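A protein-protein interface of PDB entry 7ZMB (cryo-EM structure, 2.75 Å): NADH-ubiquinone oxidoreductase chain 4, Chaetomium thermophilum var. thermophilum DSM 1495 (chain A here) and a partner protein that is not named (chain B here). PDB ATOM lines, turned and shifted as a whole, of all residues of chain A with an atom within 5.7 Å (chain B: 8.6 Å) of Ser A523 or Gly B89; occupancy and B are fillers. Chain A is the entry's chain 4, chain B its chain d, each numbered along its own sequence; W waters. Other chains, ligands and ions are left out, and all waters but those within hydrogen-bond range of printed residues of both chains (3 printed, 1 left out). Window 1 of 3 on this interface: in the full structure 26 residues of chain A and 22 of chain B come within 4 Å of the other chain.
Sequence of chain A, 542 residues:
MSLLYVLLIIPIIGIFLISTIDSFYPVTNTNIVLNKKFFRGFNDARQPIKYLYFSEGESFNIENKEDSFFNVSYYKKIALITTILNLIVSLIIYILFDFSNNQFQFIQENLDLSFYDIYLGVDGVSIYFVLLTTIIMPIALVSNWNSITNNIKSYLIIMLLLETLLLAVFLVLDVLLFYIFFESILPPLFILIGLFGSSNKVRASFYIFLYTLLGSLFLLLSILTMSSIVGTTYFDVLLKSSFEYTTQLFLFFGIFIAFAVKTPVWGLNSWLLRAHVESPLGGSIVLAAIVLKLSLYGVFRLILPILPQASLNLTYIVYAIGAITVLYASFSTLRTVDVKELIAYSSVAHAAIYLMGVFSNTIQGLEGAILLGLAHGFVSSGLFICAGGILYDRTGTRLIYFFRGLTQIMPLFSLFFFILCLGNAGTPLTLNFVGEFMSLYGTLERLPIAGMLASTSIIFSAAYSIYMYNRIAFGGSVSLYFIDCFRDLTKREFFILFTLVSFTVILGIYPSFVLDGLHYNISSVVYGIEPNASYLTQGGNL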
ATOM      1  N   ILE A 363       6.572  23.927   2.301  1.00  0.00           N
ATOM      2  CA  ILE A 363       5.966  24.390   3.540  1.00  0.00           C
ATOM      3  C   ILE A 363       4.516  23.940   3.622  1.00  0.00           C
ATOM      4  O   ILE A 363       3.974  23.772   4.718  1.00  0.00           O
ATOM      5  CB  ILE A 363       6.112  25.918   3.669  1.00  0.00           C
ATOM      6  CG1 ILE A 363       5.715  26.367   5.073  1.00  0.00           C
ATOM      7  CG2 ILE A 363       5.273  26.635   2.621  1.00  0.00           C
ATOM      8  CD1 ILE A 363       6.116  27.751   5.390  1.00  0.00           C
ATOM      9  N   LEU A 518       2.239  26.657  13.824  1.00  0.00           N
ATOM     10  CA  LEU A 518       3.123  25.771  13.093  1.00  0.00           C
ATOM     11  C   LEU A 518       4.026  26.504  12.109  1.00  0.00           C
ATOM     12  O   LEU A 518       5.080  25.973  11.753  1.00  0.00           O
ATOM     13  CB  LEU A 518       2.289  24.732  12.344  1.00  0.00           C
ATOM     14  CG  LEU A 518       2.767  23.298  12.157  1.00  0.00           C
ATOM     15  CD1 LEU A 518       3.131  22.660  13.481  1.00  0.00           C
ATOM     16  CD2 LEU A 518       1.679  22.506  11.465  1.00  0.00           C
ATOM     17  N   HIS A 519       3.666  27.724  11.711  1.00  0.00           N
ATOM     18  CA  HIS A 519       4.247  28.347  10.523  1.00  0.00           C
ATOM     19  C   HIS A 519       5.725  28.665  10.699  1.00  0.00           C
ATOM     20  O   HIS A 519       6.563  28.241   9.896  1.00  0.00           O
ATOM     21  CB  HIS A 519       3.480  29.619  10.191  1.00  0.00           C
ATOM     22  CG  HIS A 519       2.213  29.385   9.439  1.00  0.00           C
ATOM     23  ND1 HIS A 519       2.075  28.388   8.503  1.00  0.00           N
ATOM     24  CD2 HIS A 519       1.020  30.017   9.496  1.00  0.00           C
ATOM     25  CE1 HIS A 519       0.855  28.430   8.001  1.00  0.00           C
ATOM     26  NE2 HIS A 519       0.194  29.409   8.587  1.00  0.00           N
ATOM     27  N   TYR A 520       6.057  29.450  11.729  1.00  0.00           N
ATOM     28  CA  TYR A 520       7.408  29.973  11.879  1.00  0.00           C
ATOM     29  C   TYR A 520       8.417  28.861  12.134  1.00  0.00           C
ATOM     30  O   TYR A 520       9.499  28.846  11.535  1.00  0.00           O
ATOM     31  CB  TYR A 520       7.424  31.001  13.007  1.00  0.00           C
ATOM     32  CG  TYR A 520       8.762  31.633  13.287  1.00  0.00           C
ATOM     33  CD1 TYR A 520       9.230  32.686  12.518  1.00  0.00           C
ATOM     34  CD2 TYR A 520       9.549  31.185  14.327  1.00  0.00           C
ATOM     35  CE1 TYR A 520      10.444  33.264  12.778  1.00  0.00           C
ATOM     36  CE2 TYR A 520      10.764  31.756  14.592  1.00  0.00           C
ATOM     37  CZ  TYR A 520      11.204  32.794  13.822  1.00  0.00           C
ATOM     38  OH  TYR A 520      12.419  33.357  14.097  1.00  0.00           O
ATOM     39  N   ASN A 521       8.082  27.911  13.001  1.00  0.00           N
ATOM     40  CA  ASN A 521       9.029  26.848  13.315  1.00  0.00           C
ATOM     41  C   ASN A 521       9.166  25.826  12.201  1.00  0.00           C
ATOM     42  O   ASN A 521      10.213  25.180  12.094  1.00  0.00           O
ATOM     43  CB  ASN A 521       8.644  26.153  14.619  1.00  0.00           C
ATOM     44  CG  ASN A 521       8.725  27.076  15.806  1.00  0.00           C
ATOM     45  OD1 ASN A 521       7.721  27.394  16.435  1.00  0.00           O
ATOM     46  ND2 ASN A 521       9.931  27.513  16.124  1.00  0.00           N
ATOM     47  N   ILE A 522       8.139  25.649  11.370  1.00  0.00           N
ATOM     48  CA  ILE A 522       8.243  24.645  10.326  1.00  0.00           C
ATOM     49  C   ILE A 522       8.940  25.238   9.113  1.00  0.00           C
ATOM     50  O   ILE A 522       9.393  24.498   8.234  1.00  0.00           O
ATOM     51  CB  ILE A 522       6.846  24.094   9.998  1.00  0.00           C
ATOM     52  CG1 ILE A 522       6.926  22.795   9.222  1.00  0.00           C
ATOM     53  CG2 ILE A 522       6.108  25.050   9.081  1.00  0.00           C
ATOM     54  CD1 ILE A 522       5.604  22.081   9.213  1.00  0.00           C
ATOM     55  N   SER A 523       9.039  26.566   9.056  1.00  0.00           N
ATOM     56  CA  SER A 523       9.883  27.232   8.072  1.00  0.00           C
ATOM     57  C   SER A 523      11.338  26.808   8.195  1.00  0.00           C
ATOM     58  O   SER A 523      12.063  26.778   7.197  1.00  0.00           O
ATOM     59  CB  SER A 523       9.760  28.742   8.247  1.00  0.00           C
ATOM     60  OG  SER A 523      10.588  29.436   7.343  1.00  0.00           O
ATOM     61  N   SER A 524      11.782  26.481   9.405  1.00  0.00           N
ATOM     62  CA  SER A 524      13.167  26.110   9.649  1.00  0.00           C
ATOM     63  C   SER A 524      13.546  24.755   9.065  1.00  0.00           C
ATOM     64  O   SER A 524      14.739  24.455   8.979  1.00  0.00           O
ATOM     65  CB  SER A 524      13.436  26.108  11.146  1.00  0.00           C
ATOM     66  OG  SER A 524      12.568  25.208  11.807  1.00  0.00           O
ATOM     67  N   VAL A 525      12.582  23.928   8.678  1.00  0.00           N
ATOM     68  CA  VAL A 525      12.879  22.580   8.219  1.00  0.00           C
ATOM     69  C   VAL A 525      12.756  22.461   6.701  1.00  0.00           C
ATOM     70  O   VAL A 525      12.672  21.356   6.176  1.00  0.00           O
ATOM     71  CB  VAL A 525      12.018  21.530   8.944  1.00  0.00           C
ATOM     72  CG1 VAL A 525      12.146  21.690  10.445  1.00  0.00           C
ATOM     73  CG2 VAL A 525      10.578  21.628   8.533  1.00  0.00           C
ATOM     74  N   VAL A 526      12.769  23.582   5.986  1.00  0.00           N
ATOM     75  CA  VAL A 526      12.810  23.567   4.532  1.00  0.00           C
ATOM     76  C   VAL A 526      14.265  23.641   4.085  1.00  0.00           C
ATOM     77  O   VAL A 526      15.137  24.119   4.807  1.00  0.00           O
ATOM     78  CB  VAL A 526      11.984  24.720   3.929  1.00  0.00           C
ATOM     79  CG1 VAL A 526      11.796  24.531   2.423  1.00  0.00           C
ATOM     80  CG2 VAL A 526      10.648  24.856   4.633  1.00  0.00           C
ATOM     81  N   GLY A 528      16.533  24.923   0.770  1.00  0.00           N
ATOM     82  CA  GLY A 528      16.655  25.472  -0.590  1.00  0.00           C
ATOM     83  C   GLY A 528      16.691  26.980  -0.603  1.00  0.00           C
ATOM     84  O   GLY A 528      16.591  27.576   0.481  1.00  0.00           O
ATOM     85  N   ILE A 529      16.828  27.571  -1.790  1.00  0.00           N
ATOM     86  CA  ILE A 529      16.984  29.048  -1.891  1.00  0.00           C
ATOM     87  C   ILE A 529      16.420  29.500  -3.235  1.00  0.00           C
ATOM     88  O   ILE A 529      16.337  28.667  -4.144  1.00  0.00           O
ATOM     89  CB  ILE A 529      18.468  29.449  -1.769  1.00  0.00           C
ATOM     90  CG1 ILE A 529      19.352  28.659  -2.737  1.00  0.00           C
ATOM     91  CG2 ILE A 529      18.956  29.340  -0.334  1.00  0.00           C
ATOM     92  CD1 ILE A 529      20.714  29.270  -2.953  1.00  0.00           C
ATOM     93  N   PHE B  20      24.292  35.056   6.888  1.00  0.00           N
ATOM     94  CA  PHE B  20      25.265  34.310   7.676  1.00  0.00           C
ATOM     95  C   PHE B  20      26.692  34.751   7.378  1.00  0.00           C
ATOM     96  O   PHE B  20      27.642  34.044   7.727  1.00  0.00           O
ATOM     97  CB  PHE B  20      25.125  32.807   7.435  1.00  0.00           C
ATOM     98  CG  PHE B  20      23.885  32.211   8.015  1.00  0.00           C
ATOM     99  CD1 PHE B  20      23.739  32.079   9.380  1.00  0.00           C
ATOM    100  CD2 PHE B  20      22.869  31.781   7.195  1.00  0.00           C
ATOM    101  CE1 PHE B  20      22.603  31.537   9.910  1.00  0.00           C
ATOM    102  CE2 PHE B  20      21.739  31.233   7.718  1.00  0.00           C
ATOM    103  CZ  PHE B  20      21.599  31.113   9.081  1.00  0.00           C
ATOM    104  N   ALA B  34      20.352  35.312  13.209  1.00  0.00           N
ATOM    105  CA  ALA B  34      20.539  35.247  11.766  1.00  0.00           C
ATOM    106  C   ALA B  34      19.498  34.345  11.125  1.00  0.00           C
ATOM    107  O   ALA B  34      18.876  34.712  10.125  1.00  0.00           O
ATOM    108  CB  ALA B  34      21.942  34.751  11.444  1.00  0.00           C
ATOM    109  N   GLN B  35      19.285  33.160  11.702  1.00  0.00           N
ATOM    110  CA  GLN B  35      18.234  32.281  11.202  1.00  0.00           C
ATOM    111  C   GLN B  35      16.882  32.966  11.277  1.00  0.00           C
ATOM    112  O   GLN B  35      16.109  32.931  10.315  1.00  0.00           O
ATOM    113  CB  GLN B  35      18.200  30.976  11.993  1.00  0.00           C
ATOM    114  CG  GLN B  35      19.455  30.153  11.930  1.00  0.00           C
ATOM    115  CD  GLN B  35      19.563  29.188  13.080  1.00  0.00           C
ATOM    116  OE1 GLN B  35      18.989  29.407  14.136  1.00  0.00           O
ATOM    117  NE2 GLN B  35      20.310  28.112  12.884  1.00  0.00           N
ATOM    118  N   ASP B  36      16.591  33.614  12.407  1.00  0.00           N
ATOM    119  CA  ASP B  36      15.313  34.299  12.557  1.00  0.00           C
ATOM    120  C   ASP B  36      15.136  35.375  11.505  1.00  0.00           C
ATOM    121  O   ASP B  36      14.115  35.416  10.813  1.00  0.00           O
ATOM    122  CB  ASP B  36      15.194  34.929  13.935  1.00  0.00           C
ATOM    123  CG  ASP B  36      14.039  35.894  14.018  1.00  0.00           C
ATOM    124  OD1 ASP B  36      12.934  35.515  13.585  1.00  0.00           O
ATOM    125  OD2 ASP B  36      14.238  37.033  14.492  1.00  0.00           O
ATOM    126  N   ALA B  37      16.127  36.259  11.374  1.00  0.00           N
ATOM    127  CA  ALA B  37      16.067  37.386  10.406  1.00  0.00           C
ATOM    128  C   ALA B  37      15.888  36.898   8.968  1.00  0.00           C
ATOM    129  O   ALA B  37      15.163  37.566   8.217  1.00  0.00           O
ATOM    130  CB  ALA B  37      17.266  38.288  10.556  1.00  0.00           C
ATOM    131  N   ILE B  38      16.477  35.764   8.602  1.00  0.00           N
ATOM    132  CA  ILE B  38      16.384  35.328   7.178  1.00  0.00           C
ATOM    133  C   ILE B  38      14.958  34.800   7.021  1.00  0.00           C
ATOM    134  O   ILE B  38      14.355  35.025   5.959  1.00  0.00           O
ATOM    135  CB  ILE B  38      17.433  34.243   6.862  1.00  0.00           C
ATOM    136  CG1 ILE B  38      18.847  34.825   6.818  1.00  0.00           C
ATOM    137  CG2 ILE B  38      17.101  33.495   5.581  1.00  0.00           C
ATOM    138  CD1 ILE B  38      19.888  33.872   6.291  1.00  0.00           C
ATOM    139  N   ILE B  39      14.418  34.196   8.081  1.00  0.00           N
ATOM    140  CA  ILE B  39      13.035  33.741   8.037  1.00  0.00           C
ATOM    141  C   ILE B  39      12.074  34.921   7.966  1.00  0.00           C
ATOM    142  O   ILE B  39      11.014  34.828   7.334  1.00  0.00           O
ATOM    143  CB  ILE B  39      12.739  32.832   9.244  1.00  0.00           C
ATOM    144  CG1 ILE B  39      13.536  31.531   9.141  1.00  0.00           C
ATOM    145  CG2 ILE B  39      11.271  32.506   9.328  1.00  0.00           C
ATOM    146  CD1 ILE B  39      13.480  30.886   7.799  1.00  0.00           C
ATOM    147  N   ARG B  40      12.385  36.009   8.670  1.00  0.00           N
ATOM    148  CA  ARG B  40      11.484  37.194   8.740  1.00  0.00           C
ATOM    149  C   ARG B  40      11.304  37.824   7.357  1.00  0.00           C
ATOM    150  O   ARG B  40      10.182  38.253   7.057  1.00  0.00           O
ATOM    151  CB  ARG B  40      12.046  38.231   9.712  1.00  0.00           C
ATOM    152  CG  ARG B  40      12.044  37.790  11.167  1.00  0.00           C
ATOM    153  CD  ARG B  40      10.680  37.860  11.813  1.00  0.00           C
ATOM    154  NE  ARG B  40      10.695  37.155  13.081  1.00  0.00           N
ATOM    155  CZ  ARG B  40       9.705  37.164  13.958  1.00  0.00           C
ATOM    156  NH1 ARG B  40       8.609  37.858  13.711  1.00  0.00           N
ATOM    157  NH2 ARG B  40       9.818  36.482  15.080  1.00  0.00           N
ATOM    158  N   GLN B  42      11.804  36.424   4.157  1.00  0.00           N
ATOM    159  CA  GLN B  42      11.122  35.522   3.203  1.00  0.00           C
ATOM    160  C   GLN B  42       9.629  35.578   3.495  1.00  0.00           C
ATOM    161  O   GLN B  42       8.847  35.554   2.535  1.00  0.00           O
ATOM    162  CB  GLN B  42      11.642  34.093   3.359  1.00  0.00           C
ATOM    163  CG  GLN B  42      13.082  33.892   2.926  1.00  0.00           C
ATOM    164  CD  GLN B  42      13.473  32.453   3.137  1.00  0.00           C
ATOM    165  OE1 GLN B  42      12.808  31.717   3.861  1.00  0.00           O
ATOM    166  NE2 GLN B  42      14.557  32.039   2.502  1.00  0.00           N
ATOM    167  N   TRP B  43       9.266  35.701   4.772  1.00  0.00           N
ATOM    168  CA  TRP B  43       7.830  35.684   5.132  1.00  0.00           C
ATOM    169  C   TRP B  43       7.219  37.039   4.763  1.00  0.00           C
ATOM    170  O   TRP B  43       6.126  37.022   4.192  1.00  0.00           O
ATOM    171  CB  TRP B  43       7.641  35.349   6.618  1.00  0.00           C
ATOM    172  CG  TRP B  43       7.305  33.913   6.878  1.00  0.00           C
ATOM    173  CD1 TRP B  43       8.113  32.960   7.423  1.00  0.00           C
ATOM    174  CD2 TRP B  43       6.056  33.261   6.591  1.00  0.00           C
ATOM    175  NE1 TRP B  43       7.454  31.764   7.499  1.00  0.00           N
ATOM    176  CE2 TRP B  43       6.190  31.916   6.996  1.00  0.00           C
ATOM    177  CE3 TRP B  43       4.843  33.678   6.035  1.00  0.00           C
ATOM    178  CZ2 TRP B  43       5.159  30.990   6.855  1.00  0.00           C
ATOM    179  CZ3 TRP B  43       3.824  32.764   5.900  1.00  0.00           C
ATOM    180  CH2 TRP B  43       3.982  31.439   6.305  1.00  0.00           C
ATOM    181  N   LYS B  86       9.041  33.117  -1.807  1.00  0.00           N
ATOM    182  CA  LYS B  86       8.736  31.783  -1.317  1.00  0.00           C
ATOM    183  C   LYS B  86       9.545  31.534  -0.059  1.00  0.00           C
ATOM    184  O   LYS B  86      10.757  31.758  -0.051  1.00  0.00           O
ATOM    185  CB  LYS B  86       9.043  30.715  -2.367  1.00  0.00           C
ATOM    186  CG  LYS B  86       8.520  29.351  -2.011  1.00  0.00           C
ATOM    187  CD  LYS B  86       9.065  28.289  -2.948  1.00  0.00           C
ATOM    188  CE  LYS B  86       8.023  27.225  -3.257  1.00  0.00           C
ATOM    189  NZ  LYS B  86       6.959  27.730  -4.169  1.00  0.00           N
ATOM    190  N   VAL B  87       8.884  31.073   1.002  1.00  0.00           N
ATOM    191  CA  VAL B  87       9.620  30.699   2.237  1.00  0.00           C
ATOM    192  C   VAL B  87      10.484  29.478   1.903  1.00  0.00           C
ATOM    193  O   VAL B  87       9.904  28.431   1.560  1.00  0.00           O
ATOM    194  CB  VAL B  87       8.645  30.449   3.402  1.00  0.00           C
ATOM    195  CG1 VAL B  87       9.314  29.728   4.558  1.00  0.00           C
ATOM    196  CG2 VAL B  87       7.998  31.740   3.872  1.00  0.00           C
ATOM    197  N   LYS B  88      11.810  29.616   1.954  1.00  0.00           N
ATOM    198  CA  LYS B  88      12.696  28.484   1.566  1.00  0.00           C
ATOM    199  C   LYS B  88      13.546  28.055   2.762  1.00  0.00           C
ATOM    200  O   LYS B  88      14.288  27.075   2.629  1.00  0.00           O
ATOM    201  CB  LYS B  88      13.489  28.823   0.304  1.00  0.00           C
ATOM    202  CG  LYS B  88      12.714  28.731  -1.002  1.00  0.00           C
ATOM    203  CD  LYS B  88      12.110  27.369  -1.246  1.00  0.00           C
ATOM    204  CE  LYS B  88      13.133  26.270  -1.436  1.00  0.00           C
ATOM    205  NZ  LYS B  88      12.486  24.959  -1.676  1.00  0.00           N
ATOM    206  N   GLY B  89      13.412  28.756   3.890  1.00  0.00           N
ATOM    207  CA  GLY B  89      14.162  28.405   5.105  1.00  0.00           C
ATOM    208  C   GLY B  89      15.525  29.057   5.215  1.00  0.00           C
ATOM    209  O   GLY B  89      15.833  29.896   4.362  1.00  0.00           O
ATOM    210  N   TYR B  90      16.297  28.707   6.249  1.00  0.00           N
ATOM    211  CA  TYR B  90      17.636  29.305   6.496  1.00  0.00           C
ATOM    212  C   TYR B  90      18.728  28.242   6.426  1.00  0.00           C
ATOM    213  O   TYR B  90      19.880  28.590   6.673  1.00  0.00           O
ATOM    214  CB  TYR B  90      17.676  29.868   7.916  1.00  0.00           C
ATOM    215  CG  TYR B  90      17.380  28.894   9.031  1.00  0.00           C
ATOM    216  CD1 TYR B  90      18.325  27.977   9.458  1.00  0.00           C
ATOM    217  CD2 TYR B  90      16.165  28.916   9.694  1.00  0.00           C
ATOM    218  CE1 TYR B  90      18.064  27.083  10.481  1.00  0.00           C
ATOM    219  CE2 TYR B  90      15.890  28.036  10.727  1.00  0.00           C
ATOM    220  CZ  TYR B  90      16.845  27.119  11.125  1.00  0.00           C
ATOM    221  OH  TYR B  90      16.595  26.244  12.140  1.00  0.00           O
ATOM    222  N   LEU B  91      18.384  27.005   6.096  1.00  0.00           N
ATOM    223  CA  LEU B  91      19.350  25.886   6.178  1.00  0.00           C
ATOM    224  C   LEU B  91      20.279  25.848   4.963  1.00  0.00           C
ATOM    225  O   LEU B  91      21.466  25.578   5.158  1.00  0.00           O
ATOM    226  CB  LEU B  91      18.548  24.590   6.349  1.00  0.00           C
ATOM    227  CG  LEU B  91      19.363  23.329   6.626  1.00  0.00           C
ATOM    228  CD1 LEU B  91      20.203  23.495   7.884  1.00  0.00           C
ATOM    229  CD2 LEU B  91      18.447  22.125   6.753  1.00  0.00           C
ATOM    230  N   PHE B  92      19.775  26.114   3.762  1.00  0.00           N
ATOM    231  CA  PHE B  92      20.698  26.146   2.635  1.00  0.00           C
ATOM    232  C   PHE B  92      21.661  27.317   2.749  1.00  0.00           C
ATOM    233  O   PHE B  92      22.836  27.197   2.389  1.00  0.00           O
ATOM    234  CB  PHE B  92      19.932  26.198   1.318  1.00  0.00           C
ATOM    235  CG  PHE B  92      20.716  25.683   0.162  1.00  0.00           C
ATOM    236  CD1 PHE B  92      21.546  26.520  -0.554  1.00  0.00           C
ATOM    237  CD2 PHE B  92      20.646  24.355  -0.198  1.00  0.00           C
ATOM    238  CE1 PHE B  92      22.277  26.047  -1.605  1.00  0.00           C
ATOM    239  CE2 PHE B  92      21.384  23.874  -1.247  1.00  0.00           C
ATOM    240  CZ  PHE B  92      22.201  24.723  -1.953  1.00  0.00           C
ATOM    241  N   GLU B  93      21.175  28.463   3.232  1.00  0.00           N
ATOM    242  CA  GLU B  93      22.055  29.591   3.527  1.00  0.00           C
ATOM    243  C   GLU B  93      23.088  29.222   4.581  1.00  0.00           C
ATOM    244  O   GLU B  93      24.278  29.518   4.428  1.00  0.00           O
ATOM    245  CB  GLU B  93      21.232  30.781   4.014  1.00  0.00           C
ATOM    246  CG  GLU B  93      20.396  31.492   2.966  1.00  0.00           C
ATOM    247  CD  GLU B  93      21.203  32.452   2.129  1.00  0.00           C
ATOM    248  OE1 GLU B  93      22.130  33.074   2.677  1.00  0.00           O
ATOM    249  OE2 GLU B  93      20.901  32.599   0.934  1.00  0.00           O
ATOM    250  N   GLN B  94      22.652  28.567   5.654  1.00  0.00           N
ATOM    251  CA  GLN B  94      23.542  28.290   6.771  1.00  0.00           C
ATOM    252  C   GLN B  94      24.654  27.326   6.394  1.00  0.00           C
ATOM    253  O   GLN B  94      25.758  27.409   6.941  1.00  0.00           O
ATOM    254  CB  GLN B  94      22.736  27.733   7.938  1.00  0.00           C
ATOM    255  CG  GLN B  94      23.353  27.995   9.286  1.00  0.00           C
ATOM    256  CD  GLN B  94      22.590  27.344  10.400  1.00  0.00           C
ATOM    257  OE1 GLN B  94      21.455  27.711  10.684  1.00  0.00           O
ATOM    258  NE2 GLN B  94      23.206  26.366  11.043  1.00  0.00           N
HETATM  259  O   HOH W   1       8.600  25.685   0.822  1.00  0.00           O
HETATM  260  O   HOH W   2      18.201  29.026   3.206  1.00  0.00           O
HETATM  261  O   HOH W   3      15.559  26.139   6.787  1.00  0.00           O
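The side-chain hydroxyl of Tyr A520 lies close to the side-chain carboxylate of Asp B36 (2.3 Å). O of Gly A528 lies close to O of Lys B88 (3.2 Å).
OD1 of Asp B36 is in salt-bridge range of NE of Arg B40 (2.8 Å). The side-chain amide oxygen (OE1) of Gln B42 sits at hydrogen-bond distance from the backbone NH (N) of Lys B88. OE1 of Gln B42 is in hydrogen-bond range of N of Gly B89 (3.0 Å).
Trp B43 touches Ile A363. CG1 of Val B87 touches CD1 of Ile A363, 3.9 Å away. His A519 touches Trp B43. Tyr A520 touches Ile B39 (CE1 to CG2, 3.6 Å). Ser A523 touches Val B87 (OG to CG1, 3.1 Å). O of Ser A523 touches CA of Gly B89, 3.4 Å away. Tyr B90 touches Ser A524. Val A526 touches Leu B91. Phe B92 touches Gly A528 (CB to N, 3.7 Å). Ile A529 touches Phe B92.
Asn A521 touches none of the printed residues of chain B. Of chain B, only Ile B39 (3.3 Å), Trp B43 (3.9 Å), Val B87 (3.1 Å) and Gly B89 (3.4 Å) come within 4 Å of Ser A523. Printed residues of chain A within 4 Å of Asp B36: Tyr A520. Ala B37 touches none of the printed residues of chain A. Of the printed residues of chain A, Arg B40 touches Tyr A520. Gly B89 touches one residue of chain A. Printed residues of chain A within 4 Å of Tyr B90: Ser A524. The nearest residue of chain A that does not touch Gly B89 is Val A526 (4.3 Å). The nearest printed residue of chain B that does not touch Tyr A520 is Trp B43 (4.7 Å).
Of the 12 printed residues of chain A, 8 touch a printed residue of chain B. Printed residues of chain A that touch a printed residue of chain B: Ile A363, His A519, Tyr A520, Ser A523, Ser A524, Val A526, Gly A528 and Ile A529. Printed residues of chain B that touch a printed residue of chain A: Asp B36, Ile B39, Arg B40, Trp B43, Val B87, Lys B88, Gly B89, Tyr B90, Leu B91 and Phe B92. Hydrophobic or aromatic side chains of chain B that line the printed part of chain A: Ile B39, Trp B43, Val B87, Tyr B90, Leu B91 and Phe B92. Among the printed residues, no Asp or Glu carboxylate lies within 4 Å of a Lys or Arg side-chain nitrogen of the other chain.
Water W3 lies within hydrogen-bond range of N of Tyr B90 (2.7 Å), O of Val A526 (2.9 Å), O of Ser A524 (2.9 Å) and N of Leu B91 (3.0 Å). Water W2 lies within hydrogen-bond range of the backbone carbonyl oxygen (O) of Gly B89 (2.8 Å), the backbone NH (N) of Glu B93 (3.0 Å), the backbone NH (N) of Phe B92 (3.4 Å) and the backbone carbonyl oxygen (O) of Gly A528 (3.5 Å). Water W1 lies within hydrogen-bond range of N of Ile A363 (3.1 Å) and O of Val B87 (3.1 Å).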
